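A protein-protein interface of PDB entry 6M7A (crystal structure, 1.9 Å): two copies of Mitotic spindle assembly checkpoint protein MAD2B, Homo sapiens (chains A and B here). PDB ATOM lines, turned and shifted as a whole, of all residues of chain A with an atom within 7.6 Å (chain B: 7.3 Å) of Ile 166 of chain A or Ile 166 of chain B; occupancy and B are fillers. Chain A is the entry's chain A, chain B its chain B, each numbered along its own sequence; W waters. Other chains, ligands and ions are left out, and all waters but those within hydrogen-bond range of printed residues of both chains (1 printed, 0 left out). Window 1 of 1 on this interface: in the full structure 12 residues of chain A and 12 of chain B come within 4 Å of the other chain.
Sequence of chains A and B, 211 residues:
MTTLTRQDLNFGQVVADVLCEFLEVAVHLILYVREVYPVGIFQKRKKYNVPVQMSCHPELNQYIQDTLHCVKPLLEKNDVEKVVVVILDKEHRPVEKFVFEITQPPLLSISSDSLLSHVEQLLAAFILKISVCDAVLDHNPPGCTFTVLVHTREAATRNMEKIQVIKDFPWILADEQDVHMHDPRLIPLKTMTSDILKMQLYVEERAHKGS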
ATOM      1  N   GLN A  62      39.385  10.799  23.358  1.00  0.00           N
ATOM      2  CA  GLN A  62      38.005  10.667  23.815  1.00  0.00           C
ATOM      3  C   GLN A  62      37.340   9.435  23.213  1.00  0.00           C
ATOM      4  O   GLN A  62      36.585   8.733  23.899  1.00  0.00           O
ATOM      5  CB  GLN A  62      37.217  11.942  23.470  1.00  0.00           C
ATOM      6  CG  GLN A  62      35.837  12.023  24.166  1.00  0.00           C
ATOM      7  CD  GLN A  62      35.962  12.129  25.690  1.00  0.00           C
ATOM      8  OE1 GLN A  62      36.587  13.059  26.193  1.00  0.00           O
ATOM      9  NE2 GLN A  62      35.378  11.172  26.425  1.00  0.00           N
ATOM     10  N   GLN A  65      38.775   6.494  25.230  1.00  0.00           N
ATOM     11  CA  GLN A  65      38.244   6.482  26.592  1.00  0.00           C
ATOM     12  C   GLN A  65      36.768   6.101  26.607  1.00  0.00           C
ATOM     13  O   GLN A  65      36.337   5.284  27.430  1.00  0.00           O
ATOM     14  CB  GLN A  65      38.461   7.848  27.248  1.00  0.00           C
ATOM     15  CG  GLN A  65      38.449   7.809  28.764  1.00  0.00           C
ATOM     16  CD  GLN A  65      38.412   9.197  29.375  1.00  0.00           C
ATOM     17  OE1 GLN A  65      37.368   9.846  29.409  1.00  0.00           O
ATOM     18  NE2 GLN A  65      39.556   9.661  29.850  1.00  0.00           N
ATOM     19  N   ASP A  66      35.972   6.663  25.698  1.00  0.00           N
ATOM     20  CA  ASP A  66      34.552   6.316  25.690  1.00  0.00           C
ATOM     21  C   ASP A  66      34.344   4.852  25.341  1.00  0.00           C
ATOM     22  O   ASP A  66      33.500   4.179  25.947  1.00  0.00           O
ATOM     23  CB  ASP A  66      33.794   7.209  24.708  1.00  0.00           C
ATOM     24  CG  ASP A  66      33.648   8.627  25.215  1.00  0.00           C
ATOM     25  OD1 ASP A  66      33.977   8.868  26.402  1.00  0.00           O
ATOM     26  OD2 ASP A  66      33.199   9.488  24.430  1.00  0.00           O
ATOM     27  N   THR A  67      35.095   4.344  24.355  1.00  0.00           N
ATOM     28  CA  THR A  67      34.989   2.935  23.971  1.00  0.00           C
ATOM     29  C   THR A  67      35.179   2.018  25.165  1.00  0.00           C
ATOM     30  O   THR A  67      34.378   1.108  25.397  1.00  0.00           O
ATOM     31  CB  THR A  67      36.028   2.590  22.893  1.00  0.00           C
ATOM     32  OG1 THR A  67      35.719   3.291  21.694  1.00  0.00           O
ATOM     33  CG2 THR A  67      36.031   1.078  22.600  1.00  0.00           C
ATOM     34  N   LEU A  68      36.262   2.221  25.920  1.00  0.00           N
ATOM     35  CA  LEU A  68      36.556   1.323  27.031  1.00  0.00           C
ATOM     36  C   LEU A  68      35.641   1.565  28.220  1.00  0.00           C
ATOM     37  O   LEU A  68      35.316   0.621  28.954  1.00  0.00           O
ATOM     38  CB  LEU A  68      38.023   1.465  27.419  1.00  0.00           C
ATOM     39  CG  LEU A  68      38.690   0.757  26.240  1.00  0.00           C
ATOM     40  CD1 LEU A  68      40.063   1.281  25.908  1.00  0.00           C
ATOM     41  CD2 LEU A  68      38.689  -0.745  26.484  1.00  0.00           C
ATOM     42  N   HIS A  69      35.184   2.799  28.404  1.00  0.00           N
ATOM     43  CA  HIS A  69      34.238   3.047  29.483  1.00  0.00           C
ATOM     44  C   HIS A  69      32.940   2.301  29.251  1.00  0.00           C
ATOM     45  O   HIS A  69      32.274   1.885  30.204  1.00  0.00           O
ATOM     46  CB  HIS A  69      33.976   4.539  29.615  1.00  0.00           C
ATOM     47  CG  HIS A  69      35.086   5.274  30.290  1.00  0.00           C
ATOM     48  ND1 HIS A  69      36.385   4.811  30.310  1.00  0.00           N
ATOM     49  CD2 HIS A  69      35.094   6.440  30.971  1.00  0.00           C
ATOM     50  CE1 HIS A  69      37.143   5.658  30.980  1.00  0.00           C
ATOM     51  NE2 HIS A  69      36.385   6.659  31.390  1.00  0.00           N
ATOM     52  N   CYS A  70      32.566   2.122  27.994  1.00  0.00           N
ATOM     53  CA  CYS A  70      31.371   1.347  27.704  1.00  0.00           C
ATOM     54  C   CYS A  70      31.601  -0.132  27.951  1.00  0.00           C
ATOM     55  O   CYS A  70      30.667  -0.839  28.328  1.00  0.00           O
ATOM     56  CB  CYS A  70      30.966   1.548  26.243  1.00  0.00           C
ATOM     57  SG  CYS A  70      30.245   3.149  25.816  1.00  0.00           S
ATOM     58  N   LYS A 162      23.227  -2.647  27.605  1.00  0.00           N
ATOM     59  CA  LYS A 162      24.221  -2.634  28.662  1.00  0.00           C
ATOM     60  C   LYS A 162      25.494  -1.883  28.280  1.00  0.00           C
ATOM     61  O   LYS A 162      26.141  -1.247  29.130  1.00  0.00           O
ATOM     62  CB  LYS A 162      24.548  -4.064  28.966  1.00  0.00           C
ATOM     63  CG  LYS A 162      25.411  -4.196  30.070  1.00  0.00           C
ATOM     64  CD  LYS A 162      24.975  -5.445  30.714  1.00  0.00           C
ATOM     65  CE  LYS A 162      24.959  -5.253  32.153  1.00  0.00           C
ATOM     66  NZ  LYS A 162      23.718  -4.629  32.754  1.00  0.00           N
ATOM     67  N   ILE A 163      25.916  -2.018  27.028  1.00  0.00           N
ATOM     68  CA  ILE A 163      27.170  -1.408  26.612  1.00  0.00           C
ATOM     69  C   ILE A 163      27.003   0.080  26.325  1.00  0.00           C
ATOM     70  O   ILE A 163      28.000   0.813  26.271  1.00  0.00           O
ATOM     71  CB  ILE A 163      27.709  -2.171  25.391  1.00  0.00           C
ATOM     72  CG1 ILE A 163      29.219  -1.951  25.229  1.00  0.00           C
ATOM     73  CG2 ILE A 163      26.900  -1.812  24.133  1.00  0.00           C
ATOM     74  CD1 ILE A 163      29.870  -2.861  24.231  1.00  0.00           C
ATOM     75  N   GLN A 164      25.775   0.564  26.169  1.00  0.00           N
ATOM     76  CA  GLN A 164      25.562   1.946  25.729  1.00  0.00           C
ATOM     77  C   GLN A 164      25.477   2.870  26.946  1.00  0.00           C
ATOM     78  O   GLN A 164      24.428   3.392  27.328  1.00  0.00           O
ATOM     79  CB  GLN A 164      24.343   2.026  24.812  1.00  0.00           C
ATOM     80  CG  GLN A 164      24.811   1.814  23.354  1.00  0.00           C
ATOM     81  CD  GLN A 164      23.773   1.241  22.430  1.00  0.00           C
ATOM     82  OE1 GLN A 164      23.963   1.231  21.215  1.00  0.00           O
ATOM     83  NE2 GLN A 164      22.667   0.768  22.988  1.00  0.00           N
ATOM     84  N   VAL A 165      26.659   3.075  27.528  1.00  0.00           N
ATOM     85  CA  VAL A 165      26.874   3.804  28.775  1.00  0.00           C
ATOM     86  C   VAL A 165      26.940   5.313  28.538  1.00  0.00           C
ATOM     87  O   VAL A 165      26.614   6.107  29.433  1.00  0.00           O
ATOM     88  CB  VAL A 165      28.187   3.277  29.409  1.00  0.00           C
ATOM     89  CG1 VAL A 165      28.635   4.130  30.588  1.00  0.00           C
ATOM     90  CG2 VAL A 165      28.044   1.817  29.809  1.00  0.00           C
ATOM     91  N   ILE A 166      27.389   5.727  27.357  1.00  0.00           N
ATOM     92  CA  ILE A 166      27.748   7.113  27.059  1.00  0.00           C
ATOM     93  C   ILE A 166      26.746   7.671  26.064  1.00  0.00           C
ATOM     94  O   ILE A 166      26.584   7.126  24.962  1.00  0.00           O
ATOM     95  CB  ILE A 166      29.171   7.225  26.485  1.00  0.00           C
ATOM     96  CG1 ILE A 166      30.209   6.578  27.401  1.00  0.00           C
ATOM     97  CG2 ILE A 166      29.526   8.709  26.203  1.00  0.00           C
ATOM     98  CD1 ILE A 166      30.123   7.028  28.807  1.00  0.00           C
ATOM     99  N   LYS A 167      26.107   8.778  26.422  1.00  0.00           N
ATOM    100  CA  LYS A 167      25.205   9.424  25.485  1.00  0.00           C
ATOM    101  C   LYS A 167      25.958   9.797  24.216  1.00  0.00           C
ATOM    102  O   LYS A 167      27.119  10.209  24.258  1.00  0.00           O
ATOM    103  CB  LYS A 167      24.561  10.662  26.106  1.00  0.00           C
ATOM    104  CG  LYS A 167      23.940  10.441  27.485  1.00  0.00           C
ATOM    105  CD  LYS A 167      23.325   9.048  27.690  1.00  0.00           C
ATOM    106  CE  LYS A 167      22.595   8.954  29.017  1.00  0.00           C
ATOM    107  NZ  LYS A 167      21.249   8.348  28.860  1.00  0.00           N
ATOM    108  N   ASP A 168      25.302   9.605  23.083  1.00  0.00           N
ATOM    109  CA  ASP A 168      25.871   9.923  21.776  1.00  0.00           C
ATOM    110  C   ASP A 168      27.121   9.106  21.468  1.00  0.00           C
ATOM    111  O   ASP A 168      27.983   9.566  20.719  1.00  0.00           O
ATOM    112  CB  ASP A 168      26.191  11.418  21.656  1.00  0.00           C
ATOM    113  CG  ASP A 168      24.986  12.299  21.942  1.00  0.00           C
ATOM    114  OD1 ASP A 168      23.850  11.877  21.639  1.00  0.00           O
ATOM    115  OD2 ASP A 168      25.179  13.417  22.468  1.00  0.00           O
ATOM    116  N   PHE A 169      27.284   7.929  22.067  1.00  0.00           N
ATOM    117  CA  PHE A 169      28.354   6.996  21.695  1.00  0.00           C
ATOM    118  C   PHE A 169      27.737   5.617  21.468  1.00  0.00           C
ATOM    119  O   PHE A 169      28.006   4.661  22.211  1.00  0.00           O
ATOM    120  CB  PHE A 169      29.470   6.952  22.744  1.00  0.00           C
ATOM    121  CG  PHE A 169      30.760   6.376  22.215  1.00  0.00           C
ATOM    122  CD1 PHE A 169      31.695   7.189  21.587  1.00  0.00           C
ATOM    123  CD2 PHE A 169      31.014   5.006  22.309  1.00  0.00           C
ATOM    124  CE1 PHE A 169      32.874   6.654  21.071  1.00  0.00           C
ATOM    125  CE2 PHE A 169      32.195   4.456  21.800  1.00  0.00           C
ATOM    126  CZ  PHE A 169      33.116   5.265  21.175  1.00  0.00           C
ATOM    127  N   PRO A 170      26.918   5.476  20.428  1.00  0.00           N
ATOM    128  CA  PRO A 170      26.196   4.216  20.222  1.00  0.00           C
ATOM    129  C   PRO A 170      27.099   3.104  19.699  1.00  0.00           C
ATOM    130  O   PRO A 170      28.166   3.331  19.118  1.00  0.00           O
ATOM    131  CB  PRO A 170      25.115   4.586  19.199  1.00  0.00           C
ATOM    132  CG  PRO A 170      25.651   5.797  18.488  1.00  0.00           C
ATOM    133  CD  PRO A 170      26.651   6.470  19.365  1.00  0.00           C
ATOM    134  N   TRP A 171      26.659   1.878  19.957  1.00  0.00           N
ATOM    135  CA  TRP A 171      27.323   0.675  19.476  1.00  0.00           C
ATOM    136  C   TRP A 171      26.426  -0.005  18.449  1.00  0.00           C
ATOM    137  O   TRP A 171      25.216   0.217  18.419  1.00  0.00           O
ATOM    138  CB  TRP A 171      27.652  -0.288  20.636  1.00  0.00           C
ATOM    139  CG  TRP A 171      28.770   0.199  21.500  1.00  0.00           C
ATOM    140  CD1 TRP A 171      28.748   1.289  22.320  1.00  0.00           C
ATOM    141  CD2 TRP A 171      30.090  -0.362  21.617  1.00  0.00           C
ATOM    142  NE1 TRP A 171      29.961   1.429  22.964  1.00  0.00           N
ATOM    143  CE2 TRP A 171      30.806   0.436  22.538  1.00  0.00           C
ATOM    144  CE3 TRP A 171      30.728  -1.477  21.061  1.00  0.00           C
ATOM    145  CZ2 TRP A 171      32.126   0.161  22.898  1.00  0.00           C
ATOM    146  CZ3 TRP A 171      32.036  -1.748  21.420  1.00  0.00           C
ATOM    147  CH2 TRP A 171      32.724  -0.931  22.328  1.00  0.00           C
ATOM    148  N   GLN B  62      34.223   5.219  40.691  1.00  0.00           N
ATOM    149  CA  GLN B  62      33.283   5.304  39.578  1.00  0.00           C
ATOM    150  C   GLN B  62      32.338   6.487  39.723  1.00  0.00           C
ATOM    151  O   GLN B  62      31.976   7.124  38.724  1.00  0.00           O
ATOM    152  CB  GLN B  62      32.478   4.009  39.473  1.00  0.00           C
ATOM    153  CG  GLN B  62      31.659   3.929  38.180  1.00  0.00           C
ATOM    154  CD  GLN B  62      32.545   4.036  36.953  1.00  0.00           C
ATOM    155  OE1 GLN B  62      32.479   4.999  36.187  1.00  0.00           O
ATOM    156  NE2 GLN B  62      33.408   3.054  36.782  1.00  0.00           N
ATOM    157  N   GLN B  65      34.317   9.532  38.737  1.00  0.00           N
ATOM    158  CA  GLN B  65      34.525   9.481  37.289  1.00  0.00           C
ATOM    159  C   GLN B  65      33.266   9.884  36.542  1.00  0.00           C
ATOM    160  O   GLN B  65      33.306  10.723  35.627  1.00  0.00           O
ATOM    161  CB  GLN B  65      34.935   8.067  36.862  1.00  0.00           C
ATOM    162  CG  GLN B  65      36.410   7.806  36.768  1.00  0.00           C
ATOM    163  CD  GLN B  65      36.697   6.493  36.041  1.00  0.00           C
ATOM    164  OE1 GLN B  65      37.422   5.633  36.543  1.00  0.00           O
ATOM    165  NE2 GLN B  65      36.107   6.333  34.861  1.00  0.00           N
ATOM    166  N   ASP B  66      32.137   9.267  36.908  1.00  0.00           N
ATOM    167  CA  ASP B  66      30.862   9.574  36.268  1.00  0.00           C
ATOM    168  C   ASP B  66      30.517  11.046  36.408  1.00  0.00           C
ATOM    169  O   ASP B  66      30.052  11.676  35.452  1.00  0.00           O
ATOM    170  CB  ASP B  66      29.747   8.733  36.887  1.00  0.00           C
ATOM    171  CG  ASP B  66      29.851   7.263  36.533  1.00  0.00           C
ATOM    172  OD1 ASP B  66      30.653   6.929  35.631  1.00  0.00           O
ATOM    173  OD2 ASP B  66      29.124   6.453  37.163  1.00  0.00           O
ATOM    174  N   THR B  67      30.714  11.599  37.605  1.00  0.00           N
ATOM    175  CA  THR B  67      30.396  13.000  37.850  1.00  0.00           C
ATOM    176  C   THR B  67      31.157  13.907  36.897  1.00  0.00           C
ATOM    177  O   THR B  67      30.575  14.786  36.256  1.00  0.00           O
ATOM    178  CB  THR B  67      30.717  13.356  39.304  1.00  0.00           C
ATOM    179  OG1 THR B  67      29.857  12.608  40.180  1.00  0.00           O
ATOM    180  CG2 THR B  67      30.529  14.862  39.550  1.00  0.00           C
ATOM    181  N   LEU B  68      32.468  13.714  36.794  1.00  0.00           N
ATOM    182  CA  LEU B  68      33.266  14.606  35.967  1.00  0.00           C
ATOM    183  C   LEU B  68      33.117  14.323  34.486  1.00  0.00           C
ATOM    184  O   LEU B  68      33.269  15.241  33.671  1.00  0.00           O
ATOM    185  CB  LEU B  68      34.731  14.519  36.374  1.00  0.00           C
ATOM    186  CG  LEU B  68      34.843  15.098  37.773  1.00  0.00           C
ATOM    187  CD1 LEU B  68      36.099  14.605  38.398  1.00  0.00           C
ATOM    188  CD2 LEU B  68      34.808  16.616  37.721  1.00  0.00           C
ATOM    189  N   HIS B  69      32.825  13.082  34.097  1.00  0.00           N
ATOM    190  CA  HIS B  69      32.548  12.847  32.686  1.00  0.00           C
ATOM    191  C   HIS B  69      31.329  13.641  32.249  1.00  0.00           C
ATOM    192  O   HIS B  69      31.247  14.078  31.093  1.00  0.00           O
ATOM    193  CB  HIS B  69      32.330  11.358  32.423  1.00  0.00           C
ATOM    194  CG  HIS B  69      33.548  10.527  32.652  1.00  0.00           C
ATOM    195  ND1 HIS B  69      33.571   9.165  32.449  1.00  0.00           N
ATOM    196  CD2 HIS B  69      34.792  10.870  33.064  1.00  0.00           C
ATOM    197  CE1 HIS B  69      34.771   8.702  32.749  1.00  0.00           C
ATOM    198  NE2 HIS B  69      35.535   9.716  33.112  1.00  0.00           N
ATOM    199  N   CYS B  70      30.381  13.844  33.170  1.00  0.00           N
ATOM    200  CA  CYS B  70      29.188  14.624  32.855  1.00  0.00           C
ATOM    201  C   CYS B  70      29.515  16.105  32.732  1.00  0.00           C
ATOM    202  O   CYS B  70      28.912  16.806  31.914  1.00  0.00           O
ATOM    203  CB  CYS B  70      28.125  14.398  33.938  1.00  0.00           C
ATOM    204  SG  CYS B  70      27.283  12.749  33.856  1.00  0.00           S
ATOM    205  N   LYS B 162      22.273  18.386  28.536  1.00  0.00           N
ATOM    206  CA  LYS B 162      23.673  18.289  28.156  1.00  0.00           C
ATOM    207  C   LYS B 162      24.515  17.650  29.261  1.00  0.00           C
ATOM    208  O   LYS B 162      25.498  16.971  28.963  1.00  0.00           O
ATOM    209  CB  LYS B 162      24.185  19.680  27.737  1.00  0.00           C
ATOM    210  CG  LYS B 162      25.712  19.958  27.606  1.00  0.00           C
ATOM    211  CD  LYS B 162      26.655  18.827  27.124  1.00  0.00           C
ATOM    212  CE  LYS B 162      26.160  17.966  25.956  1.00  0.00           C
ATOM    213  NZ  LYS B 162      27.029  16.760  25.751  1.00  0.00           N
ATOM    214  N   ILE B 163      24.130  17.789  30.529  1.00  0.00           N
ATOM    215  CA  ILE B 163      24.963  17.207  31.583  1.00  0.00           C
ATOM    216  C   ILE B 163      24.708  15.712  31.785  1.00  0.00           C
ATOM    217  O   ILE B 163      25.536  15.030  32.400  1.00  0.00           O
ATOM    218  CB  ILE B 163      24.758  17.944  32.920  1.00  0.00           C
ATOM    219  CG1 ILE B 163      25.902  17.648  33.902  1.00  0.00           C
ATOM    220  CG2 ILE B 163      23.432  17.557  33.528  1.00  0.00           C
ATOM    221  CD1 ILE B 163      26.088  18.735  35.013  1.00  0.00           C
ATOM    222  N   GLN B 164      23.583  15.177  31.327  1.00  0.00           N
ATOM    223  CA  GLN B 164      23.244  13.793  31.660  1.00  0.00           C
ATOM    224  C   GLN B 164      23.851  12.869  30.604  1.00  0.00           C
ATOM    225  O   GLN B 164      23.183  12.309  29.737  1.00  0.00           O
ATOM    226  CB  GLN B 164      21.738  13.633  31.821  1.00  0.00           C
ATOM    227  CG  GLN B 164      21.295  14.192  33.192  1.00  0.00           C
ATOM    228  CD  GLN B 164      19.850  13.938  33.528  1.00  0.00           C
ATOM    229  OE1 GLN B 164      19.499  13.746  34.691  1.00  0.00           O
ATOM    230  NE2 GLN B 164      18.994  13.953  32.515  1.00  0.00           N
ATOM    231  N   VAL B 165      25.166  12.731  30.728  1.00  0.00           N
ATOM    232  CA  VAL B 165      26.031  12.069  29.756  1.00  0.00           C
ATOM    233  C   VAL B 165      26.143  10.565  30.019  1.00  0.00           C
ATOM    234  O   VAL B 165      26.398   9.791  29.087  1.00  0.00           O
ATOM    235  CB  VAL B 165      27.424  12.747  29.811  1.00  0.00           C
ATOM    236  CG1 VAL B 165      28.537  11.872  29.172  1.00  0.00           C
ATOM    237  CG2 VAL B 165      27.385  14.118  29.149  1.00  0.00           C
ATOM    238  N   ILE B 166      25.978  10.150  31.276  1.00  0.00           N
ATOM    239  CA  ILE B 166      26.283   8.796  31.733  1.00  0.00           C
ATOM    240  C   ILE B 166      24.974   8.070  32.048  1.00  0.00           C
ATOM    241  O   ILE B 166      24.130   8.577  32.803  1.00  0.00           O
ATOM    242  CB  ILE B 166      27.208   8.820  32.963  1.00  0.00           C
ATOM    243  CG1 ILE B 166      28.520   9.548  32.645  1.00  0.00           C
ATOM    244  CG2 ILE B 166      27.465   7.392  33.491  1.00  0.00           C
ATOM    245  CD1 ILE B 166      29.419   8.802  31.709  1.00  0.00           C
ATOM    246  N   LYS B 167      24.810   6.890  31.456  1.00  0.00           N
ATOM    247  CA  LYS B 167      23.677   6.024  31.746  1.00  0.00           C
ATOM    248  C   LYS B 167      23.514   5.812  33.251  1.00  0.00           C
ATOM    249  O   LYS B 167      24.489   5.545  33.964  1.00  0.00           O
ATOM    250  CB  LYS B 167      23.890   4.689  31.040  1.00  0.00           C
ATOM    251  CG  LYS B 167      22.882   3.603  31.349  1.00  0.00           C
ATOM    252  CD  LYS B 167      23.174   2.386  30.471  1.00  0.00           C
ATOM    253  CE  LYS B 167      22.272   1.201  30.808  1.00  0.00           C
ATOM    254  NZ  LYS B 167      22.852   0.403  31.936  1.00  0.00           N
ATOM    255  N   ASP B 168      22.275   5.945  33.729  1.00  0.00           N
ATOM    256  CA  ASP B 168      21.924   5.664  35.131  1.00  0.00           C
ATOM    257  C   ASP B 168      22.645   6.588  36.113  1.00  0.00           C
ATOM    258  O   ASP B 168      22.912   6.211  37.258  1.00  0.00           O
ATOM    259  CB  ASP B 168      22.207   4.201  35.499  1.00  0.00           C
ATOM    260  CG  ASP B 168      21.466   3.205  34.613  1.00  0.00           C
ATOM    261  OD1 ASP B 168      20.361   3.515  34.112  1.00  0.00           O
ATOM    262  OD2 ASP B 168      22.012   2.093  34.425  1.00  0.00           O
ATOM    263  N   PHE B 169      22.986   7.802  35.688  1.00  0.00           N
ATOM    264  CA  PHE B 169      23.626   8.794  36.549  1.00  0.00           C
ATOM    265  C   PHE B 169      22.909  10.120  36.345  1.00  0.00           C
ATOM    266  O   PHE B 169      23.431  11.032  35.697  1.00  0.00           O
ATOM    267  CB  PHE B 169      25.123   8.928  36.254  1.00  0.00           C
ATOM    268  CG  PHE B 169      25.888   9.630  37.349  1.00  0.00           C
ATOM    269  CD1 PHE B 169      26.346   8.927  38.457  1.00  0.00           C
ATOM    270  CD2 PHE B 169      26.142  10.989  37.273  1.00  0.00           C
ATOM    271  CE1 PHE B 169      27.040   9.564  39.470  1.00  0.00           C
ATOM    272  CE2 PHE B 169      26.826  11.635  38.289  1.00  0.00           C
ATOM    273  CZ  PHE B 169      27.267  10.918  39.393  1.00  0.00           C
ATOM    274  N   PRO B 170      21.694  10.250  36.866  1.00  0.00           N
ATOM    275  CA  PRO B 170      20.925  11.475  36.643  1.00  0.00           C
ATOM    276  C   PRO B 170      21.417  12.616  37.520  1.00  0.00           C
ATOM    277  O   PRO B 170      22.027  12.421  38.575  1.00  0.00           O
ATOM    278  CB  PRO B 170      19.492  11.069  37.014  1.00  0.00           C
ATOM    279  CG  PRO B 170      19.676   9.986  38.034  1.00  0.00           C
ATOM    280  CD  PRO B 170      20.922   9.235  37.612  1.00  0.00           C
ATOM    281  N   TRP B 171      21.139  13.826  37.055  1.00  0.00           N
ATOM    282  CA  TRP B 171      21.428  15.046  37.795  1.00  0.00           C
ATOM    283  C   TRP B 171      20.123  15.750  38.135  1.00  0.00           C
ATOM    284  O   TRP B 171      19.104  15.568  37.467  1.00  0.00           O
ATOM    285  CB  TRP B 171      22.314  16.000  36.984  1.00  0.00           C
ATOM    286  CG  TRP B 171      23.730  15.535  36.851  1.00  0.00           C
ATOM    287  CD1 TRP B 171      24.175  14.420  36.182  1.00  0.00           C
ATOM    288  CD2 TRP B 171      24.894  16.169  37.387  1.00  0.00           C
ATOM    289  NE1 TRP B 171      25.543  14.326  36.276  1.00  0.00           N
ATOM    290  CE2 TRP B 171      26.011  15.389  37.006  1.00  0.00           C
ATOM    291  CE3 TRP B 171      25.108  17.329  38.137  1.00  0.00           C
ATOM    292  CZ2 TRP B 171      27.313  15.735  37.353  1.00  0.00           C
ATOM    293  CZ3 TRP B 171      26.411  17.657  38.502  1.00  0.00           C
ATOM    294  CH2 TRP B 171      27.492  16.868  38.107  1.00  0.00           C
HETATM  295  O   HOH W   1      25.445  -0.682  31.853  1.00  0.00           O
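Of the printed residues of chain B, His 69 of chain A touches Gln 65 and His 69.
Of the printed residues of chain B, Val 165 of chain A touches Val 165 (3.7 Å), Ile 166 (3.6 Å) and Lys 167 (2.8 Å).
Ile 166 of chain A touches two residues of chain B.
Of the printed residues of chain A, His 69 of chain B touches His 69 (2.9 Å).
Of the printed residues of chain A, Val 165 of chain B touches Val 165, Ile 166 and Lys 167.
Ile 166 of chain B touches just these residues of chain A: Val 165, Ile 166 and Lys 167.
The nearest residue of chain B that does not touch Ile 166 of chain A is Lys 167 of chain B (5.0 Å).
The nearest residue of chain A that does not touch Ile 166 of chain B is His 69 of chain A (6.2 Å).
NE2 of His 69 of chain A sits at hydrogen-bond distance from NE2 of Gln 65 of chain B, at 3.5 Å.
O of Val 165 of chain A is in hydrogen-bond range of N of Lys 167 of chain B, 2.8 Å away.
The backbone NH (N) of Lys 167 of chain A is in hydrogen-bond range of the backbone carbonyl oxygen (O) of Val 165 of chain B, 2.9 Å away.
The backbone carbonyl oxygen (O) of Gln 65 of chain A is in hydrogen-bond range of a ring nitrogen (ND1) of His 69 of chain A.
The side-chain amide oxygen (OE1) of Gln 164 of chain A lies within hydrogen-bond range of the backbone NH (N) of Trp 171 of chain A, 3.0 Å away.
The side-chain sulfur (SG) of Cys 70 of chain B is in hydrogen-bond range of the backbone NH (N) of Val 165 of chain B, at 3.8 Å.
The side-chain amide oxygen (OE1) of Gln 164 of chain B is in hydrogen-bond range of the backbone NH (N) of Trp 171 of chain B (2.9 Å).
The side-chain amino group of Lys 167 of chain B lies within salt-bridge range of the side-chain carboxylate of Asp 168 of chain B, at 3.1 Å.
Printed residues of chain A that touch a printed residue of chain B: His 69, Gln 164, Val 165, Ile 166 and Lys 167.
Along chain A the printed residues that touch a printed residue of chain B span positions 69 to 167.
Of the 17 printed residues of chain B, 6 touch a printed residue of chain A.
Hydrophobic or aromatic side chains of chain B that line the printed part of chain A: His 69 and Ile 166.
Water W1 lies within hydrogen-bond range of the side-chain amino group of Lys 167 of chain B (2.8 Å) and the backbone carbonyl oxygen of Lys 162 of chain A (2.9 Å).
Among the printed residues, merely in contact across the chains: His 69 of chain A with His 69 of chain B, Gln 164 of chain A with Lys 167 of chain B, Val 165 of chain A with Val 165 of chain B, Val 165 of chain A with Ile 166 of chain B, Ile 166 of chain A with Val 165 of chain B, Ile 166 of chain A with Ile 166 of chain B, Lys 167 of chain A with Gln 164 of chain B, Lys 167 of chain A with Ile 166 of chain B and Lys 167 of chain A with Lys 167 of chain B.
His 69 of chain A touches its own counterpart, His 69 of chain B.
Val 165 of chain A touches Ile 166 of chain B, and with the chains exchanged Ile 166 of chain A touches Val 165 of chain B.
Ile 166 of chain B touches its own counterpart, Ile 166 of chain A.
Lys 167 of chain A touches Ile 166 of chain B, but with the chains exchanged Ile 166 of chain A does not touch Lys 167 of chain B (5.0 Å).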
